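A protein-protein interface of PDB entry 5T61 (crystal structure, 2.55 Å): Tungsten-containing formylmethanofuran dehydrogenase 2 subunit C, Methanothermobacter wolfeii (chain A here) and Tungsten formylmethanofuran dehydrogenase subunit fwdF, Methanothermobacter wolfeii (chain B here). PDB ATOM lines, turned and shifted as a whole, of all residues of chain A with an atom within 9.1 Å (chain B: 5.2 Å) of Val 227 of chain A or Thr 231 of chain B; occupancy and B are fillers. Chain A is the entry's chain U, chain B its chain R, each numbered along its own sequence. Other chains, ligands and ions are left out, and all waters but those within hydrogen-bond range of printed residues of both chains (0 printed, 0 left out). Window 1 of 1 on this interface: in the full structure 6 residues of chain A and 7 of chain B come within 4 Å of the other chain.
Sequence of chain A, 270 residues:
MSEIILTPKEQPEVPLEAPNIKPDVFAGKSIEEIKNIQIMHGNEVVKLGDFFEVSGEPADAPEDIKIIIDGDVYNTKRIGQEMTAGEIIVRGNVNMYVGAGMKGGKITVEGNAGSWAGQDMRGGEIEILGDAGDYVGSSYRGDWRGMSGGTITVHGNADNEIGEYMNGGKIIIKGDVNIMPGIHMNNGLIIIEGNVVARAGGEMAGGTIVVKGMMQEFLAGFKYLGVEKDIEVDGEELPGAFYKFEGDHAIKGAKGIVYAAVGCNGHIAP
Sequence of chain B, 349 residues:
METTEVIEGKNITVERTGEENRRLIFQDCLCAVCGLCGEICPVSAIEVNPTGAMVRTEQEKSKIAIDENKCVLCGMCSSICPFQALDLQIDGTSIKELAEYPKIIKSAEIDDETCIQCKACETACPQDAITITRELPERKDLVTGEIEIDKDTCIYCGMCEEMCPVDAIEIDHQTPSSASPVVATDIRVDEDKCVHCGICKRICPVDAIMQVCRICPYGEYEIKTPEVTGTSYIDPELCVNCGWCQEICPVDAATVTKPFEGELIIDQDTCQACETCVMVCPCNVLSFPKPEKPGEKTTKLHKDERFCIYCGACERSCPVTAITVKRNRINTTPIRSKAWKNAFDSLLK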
ATOM      1  N   TYR A 224       8.252   5.651  -3.518  1.00  0.00           N
ATOM      2  CA  TYR A 224       9.206   4.608  -3.188  1.00  0.00           C
ATOM      3  C   TYR A 224       9.363   3.655  -4.367  1.00  0.00           C
ATOM      4  O   TYR A 224       8.374   3.119  -4.878  1.00  0.00           O
ATOM      5  CB  TYR A 224       8.721   3.867  -1.943  1.00  0.00           C
ATOM      6  CG  TYR A 224       9.565   2.691  -1.547  1.00  0.00           C
ATOM      7  CD1 TYR A 224      10.812   2.873  -0.974  1.00  0.00           C
ATOM      8  CD2 TYR A 224       9.109   1.395  -1.737  1.00  0.00           C
ATOM      9  CE1 TYR A 224      11.586   1.799  -0.603  1.00  0.00           C
ATOM     10  CE2 TYR A 224       9.874   0.312  -1.371  1.00  0.00           C
ATOM     11  CZ  TYR A 224      11.114   0.522  -0.802  1.00  0.00           C
ATOM     12  OH  TYR A 224      11.893  -0.547  -0.432  1.00  0.00           O
ATOM     13  N   LEU A 225      10.605   3.444  -4.805  1.00  0.00           N
ATOM     14  CA  LEU A 225      10.879   2.576  -5.945  1.00  0.00           C
ATOM     15  C   LEU A 225      11.457   1.221  -5.558  1.00  0.00           C
ATOM     16  O   LEU A 225      11.569   0.346  -6.423  1.00  0.00           O
ATOM     17  CB  LEU A 225      11.838   3.263  -6.928  1.00  0.00           C
ATOM     18  CG  LEU A 225      11.410   4.609  -7.515  1.00  0.00           C
ATOM     19  CD1 LEU A 225      12.547   5.230  -8.309  1.00  0.00           C
ATOM     20  CD2 LEU A 225      10.181   4.434  -8.389  1.00  0.00           C
ATOM     21  N   GLY A 226      11.826   1.022  -4.293  1.00  0.00           N
ATOM     22  CA  GLY A 226      12.363  -0.244  -3.843  1.00  0.00           C
ATOM     23  C   GLY A 226      13.764  -0.082  -3.282  1.00  0.00           C
ATOM     24  O   GLY A 226      14.104   0.960  -2.708  1.00  0.00           O
ATOM     25  N   VAL A 227      14.574  -1.119  -3.465  1.00  0.00           N
ATOM     26  CA  VAL A 227      15.939  -1.146  -2.959  1.00  0.00           C
ATOM     27  C   VAL A 227      16.886  -1.318  -4.134  1.00  0.00           C
ATOM     28  O   VAL A 227      16.626  -2.103  -5.054  1.00  0.00           O
ATOM     29  CB  VAL A 227      16.152  -2.263  -1.915  1.00  0.00           C
ATOM     30  CG1 VAL A 227      17.627  -2.403  -1.565  1.00  0.00           C
ATOM     31  CG2 VAL A 227      15.375  -1.951  -0.649  1.00  0.00           C
ATOM     32  N   GLU A 228      17.983  -0.572  -4.094  1.00  0.00           N
ATOM     33  CA  GLU A 228      19.089  -0.712  -5.020  1.00  0.00           C
ATOM     34  C   GLU A 228      20.353  -1.019  -4.241  1.00  0.00           C
ATOM     35  O   GLU A 228      20.584  -0.471  -3.157  1.00  0.00           O
ATOM     36  CB  GLU A 228      19.309   0.540  -5.874  1.00  0.00           C
ATOM     37  CG  GLU A 228      18.940   0.357  -7.331  1.00  0.00           C
ATOM     38  CD  GLU A 228      19.529   1.439  -8.216  1.00  0.00           C
ATOM     39  OE1 GLU A 228      20.007   1.104  -9.320  1.00  0.00           O
ATOM     40  OE2 GLU A 228      19.609   2.600  -7.762  1.00  0.00           O
ATOM     41  N   LYS A 229      21.142  -1.922  -4.801  1.00  0.00           N
ATOM     42  CA  LYS A 229      22.430  -2.337  -4.281  1.00  0.00           C
ATOM     43  C   LYS A 229      23.512  -1.784  -5.189  1.00  0.00           C
ATOM     44  O   LYS A 229      23.255  -1.470  -6.353  1.00  0.00           O
ATOM     45  CB  LYS A 229      22.545  -3.866  -4.227  1.00  0.00           C
ATOM     46  CG  LYS A 229      21.288  -4.603  -3.767  1.00  0.00           C
ATOM     47  CD  LYS A 229      21.545  -6.111  -3.823  1.00  0.00           C
ATOM     48  CE  LYS A 229      21.142  -6.801  -5.116  1.00  0.00           C
ATOM     49  NZ  LYS A 229      20.767  -8.180  -4.728  1.00  0.00           N
ATOM     50  N   ASP A 230      24.722  -1.644  -4.644  1.00  0.00           N
ATOM     51  CA  ASP A 230      25.917  -1.400  -5.457  1.00  0.00           C
ATOM     52  C   ASP A 230      25.742  -0.165  -6.355  1.00  0.00           C
ATOM     53  O   ASP A 230      25.775  -0.255  -7.584  1.00  0.00           O
ATOM     54  CB  ASP A 230      26.221  -2.650  -6.290  1.00  0.00           C
ATOM     55  CG  ASP A 230      25.903  -3.949  -5.544  1.00  0.00           C
ATOM     56  OD1 ASP A 230      24.928  -4.631  -5.927  1.00  0.00           O
ATOM     57  OD2 ASP A 230      26.621  -4.304  -4.587  1.00  0.00           O
ATOM     58  N   ILE A 231      25.514   0.990  -5.729  1.00  0.00           N
ATOM     59  CA  ILE A 231      25.199   2.192  -6.488  1.00  0.00           C
ATOM     60  C   ILE A 231      26.456   2.944  -6.923  1.00  0.00           C
ATOM     61  O   ILE A 231      27.353   3.211  -6.117  1.00  0.00           O
ATOM     62  CB  ILE A 231      24.250   3.110  -5.705  1.00  0.00           C
ATOM     63  CG1 ILE A 231      23.131   2.238  -5.137  1.00  0.00           C
ATOM     64  CG2 ILE A 231      23.696   4.181  -6.624  1.00  0.00           C
ATOM     65  CD1 ILE A 231      22.093   3.003  -4.418  1.00  0.00           C
ATOM     66  N   GLY A 240      26.655  -1.486  -0.029  1.00  0.00           N
ATOM     67  CA  GLY A 240      25.464  -1.689   0.765  1.00  0.00           C
ATOM     68  C   GLY A 240      24.201  -1.409  -0.018  1.00  0.00           C
ATOM     69  O   GLY A 240      24.216  -1.060  -1.202  1.00  0.00           O
ATOM     70  N   ALA A 241      23.078  -1.563   0.678  1.00  0.00           N
ATOM     71  CA  ALA A 241      21.764  -1.389   0.082  1.00  0.00           C
ATOM     72  C   ALA A 241      21.153  -0.066   0.519  1.00  0.00           C
ATOM     73  O   ALA A 241      21.382   0.412   1.634  1.00  0.00           O
ATOM     74  CB  ALA A 241      20.834  -2.543   0.464  1.00  0.00           C
ATOM     75  N   PHE A 242      20.373   0.528  -0.382  1.00  0.00           N
ATOM     76  CA  PHE A 242      19.703   1.795  -0.125  1.00  0.00           C
ATOM     77  C   PHE A 242      18.251   1.704  -0.559  1.00  0.00           C
ATOM     78  O   PHE A 242      17.955   1.215  -1.654  1.00  0.00           O
ATOM     79  CB  PHE A 242      20.394   2.952  -0.858  1.00  0.00           C
ATOM     80  CG  PHE A 242      21.780   3.241  -0.364  1.00  0.00           C
ATOM     81  CD1 PHE A 242      22.869   2.532  -0.845  1.00  0.00           C
ATOM     82  CD2 PHE A 242      21.991   4.216   0.597  1.00  0.00           C
ATOM     83  CE1 PHE A 242      24.144   2.798  -0.382  1.00  0.00           C
ATOM     84  CE2 PHE A 242      23.261   4.484   1.065  1.00  0.00           C
ATOM     85  CZ  PHE A 242      24.339   3.776   0.576  1.00  0.00           C
ATOM     86  N   TYR A 243      17.350   2.177   0.297  1.00  0.00           N
ATOM     87  CA  TYR A 243      15.993   2.450  -0.145  1.00  0.00           C
ATOM     88  C   TYR A 243      16.024   3.580  -1.164  1.00  0.00           C
ATOM     89  O   TYR A 243      16.742   4.569  -0.992  1.00  0.00           O
ATOM     90  CB  TYR A 243      15.099   2.830   1.035  1.00  0.00           C
ATOM     91  CG  TYR A 243      14.845   1.713   2.022  1.00  0.00           C
ATOM     92  CD1 TYR A 243      14.238   0.530   1.622  1.00  0.00           C
ATOM     93  CD2 TYR A 243      15.181   1.856   3.362  1.00  0.00           C
ATOM     94  CE1 TYR A 243      13.996  -0.489   2.524  1.00  0.00           C
ATOM     95  CE2 TYR A 243      14.941   0.844   4.270  1.00  0.00           C
ATOM     96  CZ  TYR A 243      14.348  -0.326   3.846  1.00  0.00           C
ATOM     97  OH  TYR A 243      14.103  -1.336   4.746  1.00  0.00           O
ATOM     98  N   LYS A 244      15.256   3.426  -2.236  1.00  0.00           N
ATOM     99  CA  LYS A 244      15.284   4.355  -3.358  1.00  0.00           C
ATOM    100  C   LYS A 244      13.956   5.089  -3.460  1.00  0.00           C
ATOM    101  O   LYS A 244      12.895   4.459  -3.518  1.00  0.00           O
ATOM    102  CB  LYS A 244      15.582   3.622  -4.666  1.00  0.00           C
ATOM    103  CG  LYS A 244      15.659   4.541  -5.874  1.00  0.00           C
ATOM    104  CD  LYS A 244      16.183   3.792  -7.081  1.00  0.00           C
ATOM    105  CE  LYS A 244      16.417   4.728  -8.248  1.00  0.00           C
ATOM    106  NZ  LYS A 244      17.009   4.000  -9.399  1.00  0.00           N
ATOM    107  N   PHE A 245      14.022   6.417  -3.495  1.00  0.00           N
ATOM    108  CA  PHE A 245      12.846   7.267  -3.604  1.00  0.00           C
ATOM    109  C   PHE A 245      13.020   8.237  -4.761  1.00  0.00           C
ATOM    110  O   PHE A 245      14.131   8.709  -5.028  1.00  0.00           O
ATOM    111  CB  PHE A 245      12.593   8.049  -2.313  1.00  0.00           C
ATOM    112  CG  PHE A 245      12.279   7.183  -1.130  1.00  0.00           C
ATOM    113  CD1 PHE A 245      13.289   6.700  -0.313  1.00  0.00           C
ATOM    114  CD2 PHE A 245      10.967   6.855  -0.831  1.00  0.00           C
ATOM    115  CE1 PHE A 245      12.994   5.904   0.778  1.00  0.00           C
ATOM    116  CE2 PHE A 245      10.665   6.061   0.258  1.00  0.00           C
ATOM    117  CZ  PHE A 245      11.680   5.583   1.064  1.00  0.00           C
ATOM    118  N   VAL A 258      16.387  10.265  -3.786  1.00  0.00           N
ATOM    119  CA  VAL A 258      16.932  10.100  -2.442  1.00  0.00           C
ATOM    120  C   VAL A 258      17.248   8.626  -2.246  1.00  0.00           C
ATOM    121  O   VAL A 258      16.369   7.769  -2.401  1.00  0.00           O
ATOM    122  CB  VAL A 258      15.963  10.575  -1.348  1.00  0.00           C
ATOM    123  CG1 VAL A 258      16.553  10.292   0.026  1.00  0.00           C
ATOM    124  CG2 VAL A 258      15.686  12.032  -1.477  1.00  0.00           C
ATOM    125  N   TYR A 259      18.495   8.330  -1.902  1.00  0.00           N
ATOM    126  CA  TYR A 259      18.886   7.000  -1.460  1.00  0.00           C
ATOM    127  C   TYR A 259      19.061   7.034   0.052  1.00  0.00           C
ATOM    128  O   TYR A 259      19.784   7.889   0.574  1.00  0.00           O
ATOM    129  CB  TYR A 259      20.188   6.545  -2.121  1.00  0.00           C
ATOM    130  CG  TYR A 259      20.114   6.231  -3.602  1.00  0.00           C
ATOM    131  CD1 TYR A 259      19.420   5.121  -4.068  1.00  0.00           C
ATOM    132  CD2 TYR A 259      20.802   7.008  -4.529  1.00  0.00           C
ATOM    133  CE1 TYR A 259      19.374   4.820  -5.420  1.00  0.00           C
ATOM    134  CE2 TYR A 259      20.766   6.710  -5.881  1.00  0.00           C
ATOM    135  CZ  TYR A 259      20.052   5.615  -6.321  1.00  0.00           C
ATOM    136  OH  TYR A 259      20.012   5.315  -7.663  1.00  0.00           O
ATOM    137  N   ALA A 260      18.410   6.109   0.752  1.00  0.00           N
ATOM    138  CA  ALA A 260      18.518   6.017   2.202  1.00  0.00           C
ATOM    139  C   ALA A 260      18.929   4.605   2.591  1.00  0.00           C
ATOM    140  O   ALA A 260      18.301   3.634   2.161  1.00  0.00           O
ATOM    141  CB  ALA A 260      17.199   6.399   2.886  1.00  0.00           C
ATOM    142  N   ALA A 261      19.975   4.502   3.411  1.00  0.00           N
ATOM    143  CA  ALA A 261      20.535   3.206   3.777  1.00  0.00           C
ATOM    144  C   ALA A 261      19.511   2.349   4.513  1.00  0.00           C
ATOM    145  O   ALA A 261      18.808   2.820   5.409  1.00  0.00           O
ATOM    146  CB  ALA A 261      21.781   3.391   4.643  1.00  0.00           C
ATOM    147  N   VAL A 262      19.446   1.071   4.129  1.00  0.00           N
ATOM    148  CA  VAL A 262      18.414   0.170   4.635  1.00  0.00           C
ATOM    149  C   VAL A 262      18.565  -0.044   6.138  1.00  0.00           C
ATOM    150  O   VAL A 262      17.572  -0.126   6.872  1.00  0.00           O
ATOM    151  CB  VAL A 262      18.459  -1.163   3.864  1.00  0.00           C
ATOM    152  CG1 VAL A 262      17.550  -2.200   4.510  1.00  0.00           C
ATOM    153  CG2 VAL A 262      18.085  -0.951   2.407  1.00  0.00           C
ATOM    154  N   GLY A 263      19.807  -0.147   6.616  1.00  0.00           N
ATOM    155  CA  GLY A 263      20.045  -0.501   8.007  1.00  0.00           C
ATOM    156  C   GLY A 263      19.356   0.400   9.016  1.00  0.00           C
ATOM    157  O   GLY A 263      18.925  -0.061  10.077  1.00  0.00           O
ATOM    158  N   ASN A 265      16.786   2.892   8.159  1.00  0.00           N
ATOM    159  CA  ASN A 265      15.680   3.666   7.599  1.00  0.00           C
ATOM    160  C   ASN A 265      14.453   2.811   7.293  1.00  0.00           C
ATOM    161  O   ASN A 265      13.672   3.148   6.394  1.00  0.00           O
ATOM    162  CB  ASN A 265      16.111   4.420   6.337  1.00  0.00           C
ATOM    163  CG  ASN A 265      17.097   5.533   6.631  1.00  0.00           C
ATOM    164  OD1 ASN A 265      16.720   6.596   7.124  1.00  0.00           O
ATOM    165  ND2 ASN A 265      18.367   5.294   6.328  1.00  0.00           N
ATOM    166  N   ALA A 269      10.375   3.463   4.892  1.00  0.00           N
ATOM    167  CA  ALA A 269       9.700   2.671   3.871  1.00  0.00           C
ATOM    168  C   ALA A 269       8.310   2.243   4.331  1.00  0.00           C
ATOM    169  O   ALA A 269       7.449   1.909   3.514  1.00  0.00           O
ATOM    170  CB  ALA A 269      10.540   1.454   3.510  1.00  0.00           C
ATOM    171  N   ASP B 112      20.472 -13.521  -7.123  1.00  0.00           N
ATOM    172  CA  ASP B 112      19.347 -12.649  -7.445  1.00  0.00           C
ATOM    173  C   ASP B 112      18.637 -13.053  -8.729  1.00  0.00           C
ATOM    174  O   ASP B 112      17.455 -12.733  -8.893  1.00  0.00           O
ATOM    175  CB  ASP B 112      19.820 -11.200  -7.557  1.00  0.00           C
ATOM    176  CG  ASP B 112      20.262 -10.628  -6.228  1.00  0.00           C
ATOM    177  OD1 ASP B 112      19.426 -10.570  -5.299  1.00  0.00           O
ATOM    178  OD2 ASP B 112      21.440 -10.226  -6.108  1.00  0.00           O
ATOM    179  N   GLN B 117      11.576 -13.822  -5.155  1.00  0.00           N
ATOM    180  CA  GLN B 117      10.983 -12.793  -4.294  1.00  0.00           C
ATOM    181  C   GLN B 117       9.775 -13.303  -3.510  1.00  0.00           C
ATOM    182  O   GLN B 117       8.788 -12.584  -3.350  1.00  0.00           O
ATOM    183  CB  GLN B 117      10.597 -11.554  -5.103  1.00  0.00           C
ATOM    184  CG  GLN B 117      11.662 -10.488  -5.183  1.00  0.00           C
ATOM    185  CD  GLN B 117      12.831 -10.858  -6.055  1.00  0.00           C
ATOM    186  OE1 GLN B 117      13.981 -10.605  -5.702  1.00  0.00           O
ATOM    187  NE2 GLN B 117      12.550 -11.468  -7.199  1.00  0.00           N
ATOM    188  N   THR B 131      16.569  -8.259   3.657  1.00  0.00           N
ATOM    189  CA  THR B 131      15.529  -7.441   3.050  1.00  0.00           C
ATOM    190  C   THR B 131      15.195  -8.006   1.674  1.00  0.00           C
ATOM    191  O   THR B 131      16.093  -8.200   0.848  1.00  0.00           O
ATOM    192  CB  THR B 131      15.984  -5.987   2.932  1.00  0.00           C
ATOM    193  OG1 THR B 131      16.351  -5.494   4.230  1.00  0.00           O
ATOM    194  CG2 THR B 131      14.858  -5.120   2.378  1.00  0.00           C
ATOM    195  N   ILE B 132      13.914  -8.283   1.432  1.00  0.00           N
ATOM    196  CA  ILE B 132      13.429  -8.696   0.116  1.00  0.00           C
ATOM    197  C   ILE B 132      12.369  -7.700  -0.335  1.00  0.00           C
ATOM    198  O   ILE B 132      11.371  -7.487   0.366  1.00  0.00           O
ATOM    199  CB  ILE B 132      12.852 -10.120   0.124  1.00  0.00           C
ATOM    200  CG1 ILE B 132      13.880 -11.142   0.619  1.00  0.00           C
ATOM    201  CG2 ILE B 132      12.377 -10.495  -1.275  1.00  0.00           C
ATOM    202  CD1 ILE B 132      15.051 -11.329  -0.315  1.00  0.00           C
ATOM    203  N   THR B 133      12.583  -7.093  -1.498  1.00  0.00           N
ATOM    204  CA  THR B 133      11.597  -6.231  -2.133  1.00  0.00           C
ATOM    205  C   THR B 133      10.966  -6.948  -3.317  1.00  0.00           C
ATOM    206  O   THR B 133      11.601  -7.784  -3.960  1.00  0.00           O
ATOM    207  CB  THR B 133      12.219  -4.929  -2.634  1.00  0.00           C
ATOM    208  OG1 THR B 133      13.270  -5.234  -3.562  1.00  0.00           O
ATOM    209  CG2 THR B 133      12.770  -4.126  -1.477  1.00  0.00           C
ATOM    210  N   THR B 229       9.422  -8.306 -10.251  1.00  0.00           N
ATOM    211  CA  THR B 229      10.794  -7.881 -10.015  1.00  0.00           C
ATOM    212  C   THR B 229      11.034  -7.588  -8.538  1.00  0.00           C
ATOM    213  O   THR B 229      10.105  -7.471  -7.734  1.00  0.00           O
ATOM    214  CB  THR B 229      11.134  -6.654 -10.873  1.00  0.00           C
ATOM    215  OG1 THR B 229      10.655  -5.462 -10.230  1.00  0.00           O
ATOM    216  CG2 THR B 229      10.560  -6.781 -12.276  1.00  0.00           C
ATOM    217  N   GLY B 230      12.310  -7.472  -8.196  1.00  0.00           N
ATOM    218  CA  GLY B 230      12.721  -7.098  -6.857  1.00  0.00           C
ATOM    219  C   GLY B 230      14.193  -7.391  -6.670  1.00  0.00           C
ATOM    220  O   GLY B 230      14.886  -7.834  -7.592  1.00  0.00           O
ATOM    221  N   THR B 231      14.667  -7.133  -5.452  1.00  0.00           N
ATOM    222  CA  THR B 231      16.064  -7.373  -5.102  1.00  0.00           C
ATOM    223  C   THR B 231      16.131  -7.966  -3.701  1.00  0.00           C
ATOM    224  O   THR B 231      15.119  -8.108  -3.009  1.00  0.00           O
ATOM    225  CB  THR B 231      16.910  -6.090  -5.175  1.00  0.00           C
ATOM    226  OG1 THR B 231      16.417  -5.129  -4.232  1.00  0.00           O
ATOM    227  CG2 THR B 231      16.894  -5.484  -6.576  1.00  0.00           C
ATOM    228  N   SER B 232      17.347  -8.310  -3.285  1.00  0.00           N
ATOM    229  CA  SER B 232      17.607  -8.916  -1.988  1.00  0.00           C
ATOM    230  C   SER B 232      18.795  -8.223  -1.339  1.00  0.00           C
ATOM    231  O   SER B 232      19.647  -7.655  -2.022  1.00  0.00           O
ATOM    232  CB  SER B 232      17.906 -10.410  -2.119  1.00  0.00           C
ATOM    233  OG  SER B 232      19.193 -10.614  -2.673  1.00  0.00           O
ATOM    234  N   TYR B 233      18.853  -8.286  -0.012  1.00  0.00           N
ATOM    235  CA  TYR B 233      19.987  -7.730   0.710  1.00  0.00           C
ATOM    236  C   TYR B 233      20.163  -8.456   2.032  1.00  0.00           C
ATOM    237  O   TYR B 233      19.213  -8.576   2.811  1.00  0.00           O
ATOM    238  CB  TYR B 233      19.825  -6.229   0.965  1.00  0.00           C
ATOM    239  CG  TYR B 233      20.933  -5.649   1.820  1.00  0.00           C
ATOM    240  CD1 TYR B 233      22.260  -5.701   1.405  1.00  0.00           C
ATOM    241  CD2 TYR B 233      20.655  -5.044   3.040  1.00  0.00           C
ATOM    242  CE1 TYR B 233      23.278  -5.170   2.181  1.00  0.00           C
ATOM    243  CE2 TYR B 233      21.665  -4.507   3.822  1.00  0.00           C
ATOM    244  CZ  TYR B 233      22.975  -4.573   3.388  1.00  0.00           C
ATOM    245  OH  TYR B 233      23.979  -4.041   4.167  1.00  0.00           O
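Tyr 224 of chain A touches Thr 133 of chain B (OH to CG2, 3.8 Å).
Val 227 of chain A touches Thr 133 of chain B.
Tyr 233 of chain B touches Ala 241 of chain A (CG to CB, 3.4 Å).
Thr 131 of chain B touches Val 262 of chain A.
Of the 10 printed residues of chain B, 6 touch a printed residue of chain A.
Along chain A the printed residues that touch a printed residue of chain B span positions 224 to 262.
Among the printed residues, 7 pairs touch across the chains.
The backbone carbonyl oxygen (O) of Ala 241 of chain A is in hydrogen-bond range of the backbone NH (N) of Val 262 of chain A (3.2 Å).
OD1 of Asp 112 of chain B sits at hydrogen-bond distance from OG of Ser 232 of chain B (2.6 Å).
N of Thr 131 of chain B sits at hydrogen-bond distance from O of Tyr 233 of chain B (2.8 Å).
N of Thr 231 of chain B sits at hydrogen-bond distance from OG1 of Thr 133 of chain B.
Of the printed residues of chain B, Tyr 224 of chain A touches Thr 133 (3.8 Å).
Val 227 of chain A touches just these residues of chain B: Thr 133 and Thr 231.
Asp 230 of chain A touches none of the printed residues of chain B.
Printed residues of chain A within 4 Å of Thr 131 of chain B: Val 262.
Thr 133 of chain B touches just these residues of chain A: Tyr 224 (3.8 Å) and Val 227 (3.5 Å).
Thr 229 of chain B touches none of the printed residues of chain A.
Of the printed residues of chain A, Thr 231 of chain B touches Val 227.
Of chain A, only Lys 229 (3.0 Å) comes within 4 Å of Ser 232 of chain B.
The nearest residue of chain A that does not touch Thr 231 of chain B is Lys 229 of chain A (4.3 Å).
The nearest printed residue of chain A that does not touch Asp 112 of chain B is Asp 230 of chain A (6.6 Å).
OG1 of Thr 231 of chain B lies within hydrogen-bond range of O of Val 227 of chain A (3.1 Å).
The side-chain amino group (NZ) of Lys 229 of chain A lies within salt-bridge range of the side-chain carboxylate (OD2) of Asp 112 of chain B, 2.6 Å away.
The backbone carbonyl oxygen (O) of Ser 232 of chain B is in hydrogen-bond range of the side-chain amino group (NZ) of Lys 229 of chain A (3.0 Å).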
